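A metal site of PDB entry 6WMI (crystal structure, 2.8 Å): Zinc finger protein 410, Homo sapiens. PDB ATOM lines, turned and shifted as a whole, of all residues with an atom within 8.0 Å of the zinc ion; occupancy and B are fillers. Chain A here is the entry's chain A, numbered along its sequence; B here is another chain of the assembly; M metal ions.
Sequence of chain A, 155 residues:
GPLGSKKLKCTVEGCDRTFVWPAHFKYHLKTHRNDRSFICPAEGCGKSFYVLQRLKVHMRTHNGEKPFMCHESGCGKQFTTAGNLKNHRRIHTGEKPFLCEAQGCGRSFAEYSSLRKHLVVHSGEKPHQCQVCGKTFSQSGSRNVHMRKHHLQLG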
ATOM      1  N   LEU A  99      28.677  -4.474   9.522  1.00  0.00           N
ATOM      2  CA  LEU A  99      27.552  -5.023   8.780  1.00  0.00           C
ATOM      3  C   LEU A  99      27.046  -6.312   9.423  1.00  0.00           C
ATOM      4  O   LEU A  99      27.838  -7.166   9.831  1.00  0.00           O
ATOM      5  CB  LEU A  99      27.947  -5.294   7.331  1.00  0.00           C
ATOM      6  CG  LEU A  99      28.918  -4.286   6.688  1.00  0.00           C
ATOM      7  CD1 LEU A  99      29.332  -4.732   5.278  1.00  0.00           C
ATOM      8  CD2 LEU A  99      28.322  -2.875   6.650  1.00  0.00           C
ATOM      9  N   CYS A 100      25.723  -6.451   9.505  1.00  0.00           N
ATOM     10  CA  CYS A 100      25.104  -7.661  10.026  1.00  0.00           C
ATOM     11  C   CYS A 100      25.168  -8.754   8.974  1.00  0.00           C
ATOM     12  O   CYS A 100      24.569  -8.618   7.896  1.00  0.00           O
ATOM     13  CB  CYS A 100      23.661  -7.389  10.444  1.00  0.00           C
ATOM     14  SG  CYS A 100      22.768  -8.849  11.081  1.00  0.00           S
ATOM     15  N   GLU A 101      25.873  -9.844   9.280  1.00  0.00           N
ATOM     16  CA  GLU A 101      26.043 -10.960   8.366  1.00  0.00           C
ATOM     17  C   GLU A 101      24.910 -11.976   8.451  1.00  0.00           C
ATOM     18  O   GLU A 101      25.086 -13.120   8.018  1.00  0.00           O
ATOM     19  CB  GLU A 101      27.387 -11.636   8.611  1.00  0.00           C
ATOM     20  CG  GLU A 101      28.583 -10.749   8.314  1.00  0.00           C
ATOM     21  CD  GLU A 101      29.908 -11.395   8.669  1.00  0.00           C
ATOM     22  OE1 GLU A 101      29.882 -12.449   9.347  1.00  0.00           O
ATOM     23  OE2 GLU A 101      30.962 -10.865   8.264  1.00  0.00           O
ATOM     24  N   ALA A 102      23.753 -11.592   9.006  1.00  0.00           N
ATOM     25  CA  ALA A 102      22.610 -12.481   9.025  1.00  0.00           C
ATOM     26  C   ALA A 102      22.153 -12.768   7.593  1.00  0.00           C
ATOM     27  O   ALA A 102      22.606 -12.154   6.627  1.00  0.00           O
ATOM     28  CB  ALA A 102      21.467 -11.881   9.830  1.00  0.00           C
ATOM     29  N   GLN A 103      21.226 -13.725   7.471  1.00  0.00           N
ATOM     30  CA  GLN A 103      20.863 -14.221   6.146  1.00  0.00           C
ATOM     31  C   GLN A 103      20.134 -13.151   5.325  1.00  0.00           C
ATOM     32  O   GLN A 103      20.495 -12.895   4.179  1.00  0.00           O
ATOM     33  CB  GLN A 103      20.009 -15.479   6.288  1.00  0.00           C
ATOM     34  CG  GLN A 103      20.391 -16.602   5.326  1.00  0.00           C
ATOM     35  CD  GLN A 103      20.085 -16.273   3.881  1.00  0.00           C
ATOM     36  OE1 GLN A 103      19.178 -15.496   3.581  1.00  0.00           O
ATOM     37  NE2 GLN A 103      20.850 -16.864   2.970  1.00  0.00           N
ATOM     38  N   GLY A 104      19.125 -12.505   5.911  1.00  0.00           N
ATOM     39  CA  GLY A 104      18.327 -11.570   5.139  1.00  0.00           C
ATOM     40  C   GLY A 104      18.221 -10.174   5.729  1.00  0.00           C
ATOM     41  O   GLY A 104      17.270  -9.454   5.431  1.00  0.00           O
ATOM     42  N   CYS A 105      19.192  -9.783   6.548  1.00  0.00           N
ATOM     43  CA  CYS A 105      19.118  -8.497   7.239  1.00  0.00           C
ATOM     44  C   CYS A 105      19.856  -7.395   6.468  1.00  0.00           C
ATOM     45  O   CYS A 105      19.238  -6.407   6.047  1.00  0.00           O
ATOM     46  CB  CYS A 105      19.682  -8.626   8.657  1.00  0.00           C
ATOM     47  SG  CYS A 105      19.386  -7.194   9.694  1.00  0.00           S
ATOM     48  N   GLY A 106      21.161  -7.550   6.293  1.00  0.00           N
ATOM     49  CA  GLY A 106      21.948  -6.579   5.545  1.00  0.00           C
ATOM     50  C   GLY A 106      21.965  -5.186   6.131  1.00  0.00           C
ATOM     51  O   GLY A 106      22.021  -4.202   5.378  1.00  0.00           O
ATOM     52  N   ARG A 107      21.908  -5.068   7.454  1.00  0.00           N
ATOM     53  CA  ARG A 107      21.915  -3.776   8.120  1.00  0.00           C
ATOM     54  C   ARG A 107      23.318  -3.431   8.595  1.00  0.00           C
ATOM     55  O   ARG A 107      24.099  -4.309   8.985  1.00  0.00           O
ATOM     56  CB  ARG A 107      20.938  -3.778   9.302  1.00  0.00           C
ATOM     57  CG  ARG A 107      20.680  -2.398   9.889  1.00  0.00           C
ATOM     58  CD  ARG A 107      19.467  -2.397  10.809  1.00  0.00           C
ATOM     59  NE  ARG A 107      19.107  -1.057  11.235  1.00  0.00           N
ATOM     60  CZ  ARG A 107      18.008  -0.743  11.907  1.00  0.00           C
ATOM     61  NH1 ARG A 107      17.138  -1.695  12.229  1.00  0.00           N
ATOM     62  NH2 ARG A 107      17.765   0.518  12.249  1.00  0.00           N
ATOM     63  N   SER A 108      23.658  -2.148   8.547  1.00  0.00           N
ATOM     64  CA  SER A 108      24.961  -1.648   8.951  1.00  0.00           C
ATOM     65  C   SER A 108      24.826  -0.771  10.184  1.00  0.00           C
ATOM     66  O   SER A 108      23.750  -0.242  10.486  1.00  0.00           O
ATOM     67  CB  SER A 108      25.615  -0.860   7.821  1.00  0.00           C
ATOM     68  OG  SER A 108      24.746   0.137   7.325  1.00  0.00           O
ATOM     69  N   PHE A 109      25.938  -0.619  10.915  1.00  0.00           N
ATOM     70  CA  PHE A 109      25.943   0.119  12.173  1.00  0.00           C
ATOM     71  C   PHE A 109      27.185   0.973  12.289  1.00  0.00           C
ATOM     72  O   PHE A 109      28.233   0.697  11.695  1.00  0.00           O
ATOM     73  CB  PHE A 109      25.860  -0.841  13.371  1.00  0.00           C
ATOM     74  CG  PHE A 109      24.527  -1.508  13.511  1.00  0.00           C
ATOM     75  CD1 PHE A 109      23.532  -0.937  14.292  1.00  0.00           C
ATOM     76  CD2 PHE A 109      24.254  -2.700  12.851  1.00  0.00           C
ATOM     77  CE1 PHE A 109      22.290  -1.540  14.407  1.00  0.00           C
ATOM     78  CE2 PHE A 109      23.026  -3.306  12.967  1.00  0.00           C
ATOM     79  CZ  PHE A 109      22.040  -2.724  13.751  1.00  0.00           C
ATOM     80  N   LEU A 115      26.273  -3.176  16.713  1.00  0.00           N
ATOM     81  CA  LEU A 115      26.026  -4.448  16.029  1.00  0.00           C
ATOM     82  C   LEU A 115      25.866  -5.587  17.031  1.00  0.00           C
ATOM     83  O   LEU A 115      25.015  -6.459  16.850  1.00  0.00           O
ATOM     84  CB  LEU A 115      27.159  -4.750  15.055  1.00  0.00           C
ATOM     85  CG  LEU A 115      27.118  -6.081  14.289  1.00  0.00           C
ATOM     86  CD1 LEU A 115      25.744  -6.352  13.701  1.00  0.00           C
ATOM     87  CD2 LEU A 115      28.160  -6.078  13.186  1.00  0.00           C
ATOM     88  N   HIS A 118      22.548  -5.536  18.374  1.00  0.00           N
ATOM     89  CA  HIS A 118      21.568  -5.910  17.362  1.00  0.00           C
ATOM     90  C   HIS A 118      21.461  -7.416  17.206  1.00  0.00           C
ATOM     91  O   HIS A 118      20.382  -7.933  16.912  1.00  0.00           O
ATOM     92  CB  HIS A 118      21.922  -5.260  16.024  1.00  0.00           C
ATOM     93  CG  HIS A 118      21.125  -5.777  14.858  1.00  0.00           C
ATOM     94  ND1 HIS A 118      19.853  -5.349  14.568  1.00  0.00           N
ATOM     95  CD2 HIS A 118      21.447  -6.687  13.906  1.00  0.00           C
ATOM     96  CE1 HIS A 118      19.412  -5.974  13.494  1.00  0.00           C
ATOM     97  NE2 HIS A 118      20.358  -6.793  13.075  1.00  0.00           N
ATOM     98  N   LEU A 119      22.565  -8.143  17.390  1.00  0.00           N
ATOM     99  CA  LEU A 119      22.566  -9.588  17.169  1.00  0.00           C
ATOM    100  C   LEU A 119      21.621 -10.321  18.116  1.00  0.00           C
ATOM    101  O   LEU A 119      21.239 -11.459  17.838  1.00  0.00           O
ATOM    102  CB  LEU A 119      23.983 -10.147  17.285  1.00  0.00           C
ATOM    103  CG  LEU A 119      24.944  -9.767  16.161  1.00  0.00           C
ATOM    104  CD1 LEU A 119      26.367 -10.236  16.466  1.00  0.00           C
ATOM    105  CD2 LEU A 119      24.479 -10.324  14.818  1.00  0.00           C
ATOM    106  N   VAL A 120      21.245  -9.703  19.236  1.00  0.00           N
ATOM    107  CA  VAL A 120      20.279 -10.321  20.132  1.00  0.00           C
ATOM    108  C   VAL A 120      18.856 -10.197  19.601  1.00  0.00           C
ATOM    109  O   VAL A 120      17.966 -10.938  20.056  1.00  0.00           O
ATOM    110  CB  VAL A 120      20.382  -9.738  21.555  1.00  0.00           C
ATOM    111  CG1 VAL A 120      21.848  -9.613  21.972  1.00  0.00           C
ATOM    112  CG2 VAL A 120      19.671  -8.397  21.633  1.00  0.00           C
ATOM    113  N   VAL A 121      18.608  -9.286  18.663  1.00  0.00           N
ATOM    114  CA  VAL A 121      17.285  -9.209  18.047  1.00  0.00           C
ATOM    115  C   VAL A 121      17.042 -10.427  17.161  1.00  0.00           C
ATOM    116  O   VAL A 121      15.906 -10.899  17.035  1.00  0.00           O
ATOM    117  CB  VAL A 121      17.125  -7.898  17.248  1.00  0.00           C
ATOM    118  N   HIS A 122      18.102 -10.957  16.543  1.00  0.00           N
ATOM    119  CA  HIS A 122      17.970 -12.161  15.720  1.00  0.00           C
ATOM    120  C   HIS A 122      17.968 -13.418  16.587  1.00  0.00           C
ATOM    121  O   HIS A 122      17.144 -14.315  16.387  1.00  0.00           O
ATOM    122  CB  HIS A 122      19.084 -12.223  14.671  1.00  0.00           C
ATOM    123  CG  HIS A 122      19.029 -11.130  13.660  1.00  0.00           C
ATOM    124  ND1 HIS A 122      17.914 -10.352  13.455  1.00  0.00           N
ATOM    125  CD2 HIS A 122      19.966 -10.674  12.796  1.00  0.00           C
ATOM    126  CE1 HIS A 122      18.150  -9.466  12.509  1.00  0.00           C
ATOM    127  NE2 HIS A 122      19.395  -9.640  12.081  1.00  0.00           N
ATOM    128  P    DA B   4      18.403  -2.837  16.948  1.00  0.00           P
ATOM    129  OP1  DA B   4      18.364  -3.637  15.710  1.00  0.00           O
ATOM    130  OP2  DA B   4      19.266  -3.266  18.078  1.00  0.00           O
ATOM    131  O5'  DA B   4      18.735  -1.313  16.590  1.00  0.00           O
ATOM    132  C5'  DA B   4      17.842  -0.601  15.759  1.00  0.00           C
ATOM    133  C4'  DA B   4      18.136   0.884  15.785  1.00  0.00           C
ATOM    134  O4'  DA B   4      17.922   1.415  17.115  1.00  0.00           O
ATOM    135  C3'  DA B   4      19.550   1.289  15.392  1.00  0.00           C
ATOM    136  O3'  DA B   4      19.500   2.489  14.608  1.00  0.00           O
ATOM    137  C2'  DA B   4      20.238   1.503  16.753  1.00  0.00           C
ATOM    138  C1'  DA B   4      19.088   2.032  17.597  1.00  0.00           C
ATOM    139  N9   DA B   4      19.191   1.723  19.023  1.00  0.00           N
ATOM    140  C8   DA B   4      19.525   0.518  19.572  1.00  0.00           C
ATOM    141  N7   DA B   4      19.508   0.522  20.889  1.00  0.00           N
ATOM    142  C5   DA B   4      19.120   1.812  21.214  1.00  0.00           C
ATOM    143  C6   DA B   4      18.925   2.456  22.449  1.00  0.00           C
ATOM    144  N6   DA B   4      19.080   1.849  23.629  1.00  0.00           N
ATOM    145  N1   DA B   4      18.547   3.754  22.421  1.00  0.00           N
ATOM    146  C2   DA B   4      18.392   4.353  21.234  1.00  0.00           C
ATOM    147  N3   DA B   4      18.551   3.854  20.016  1.00  0.00           N
ATOM    148  C4   DA B   4      18.920   2.563  20.079  1.00  0.00           C
HETATM  149 ZN    ZN M   1      20.581  -8.080  11.467  1.00  0.00          ZN
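The side-chain sulfur (SG) of Cys 100 sits close to the backbone NH (N) of Ala 102 (3.6 Å). OP1 of DA 4 of chain B is in hydrogen-bond range of ND1 of His 118 (2.5 Å). N of Cys 100 lies within hydrogen-bond range of O of Arg 107.
Of the 18 residues printed, 4 come within 4 Å of the zinc ion. The nearest printed residue that does not touch the zinc ion is Ala 102 (4.2 Å).
The zinc ion is bound by NE2 of His 122 (2.1 Å), NE2 of His 118 (2.1 Å), SG of Cys 105 (2.3 Å) and SG of Cys 100 (2.4 Å). The zinc ion has four donor atoms within binding distance.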
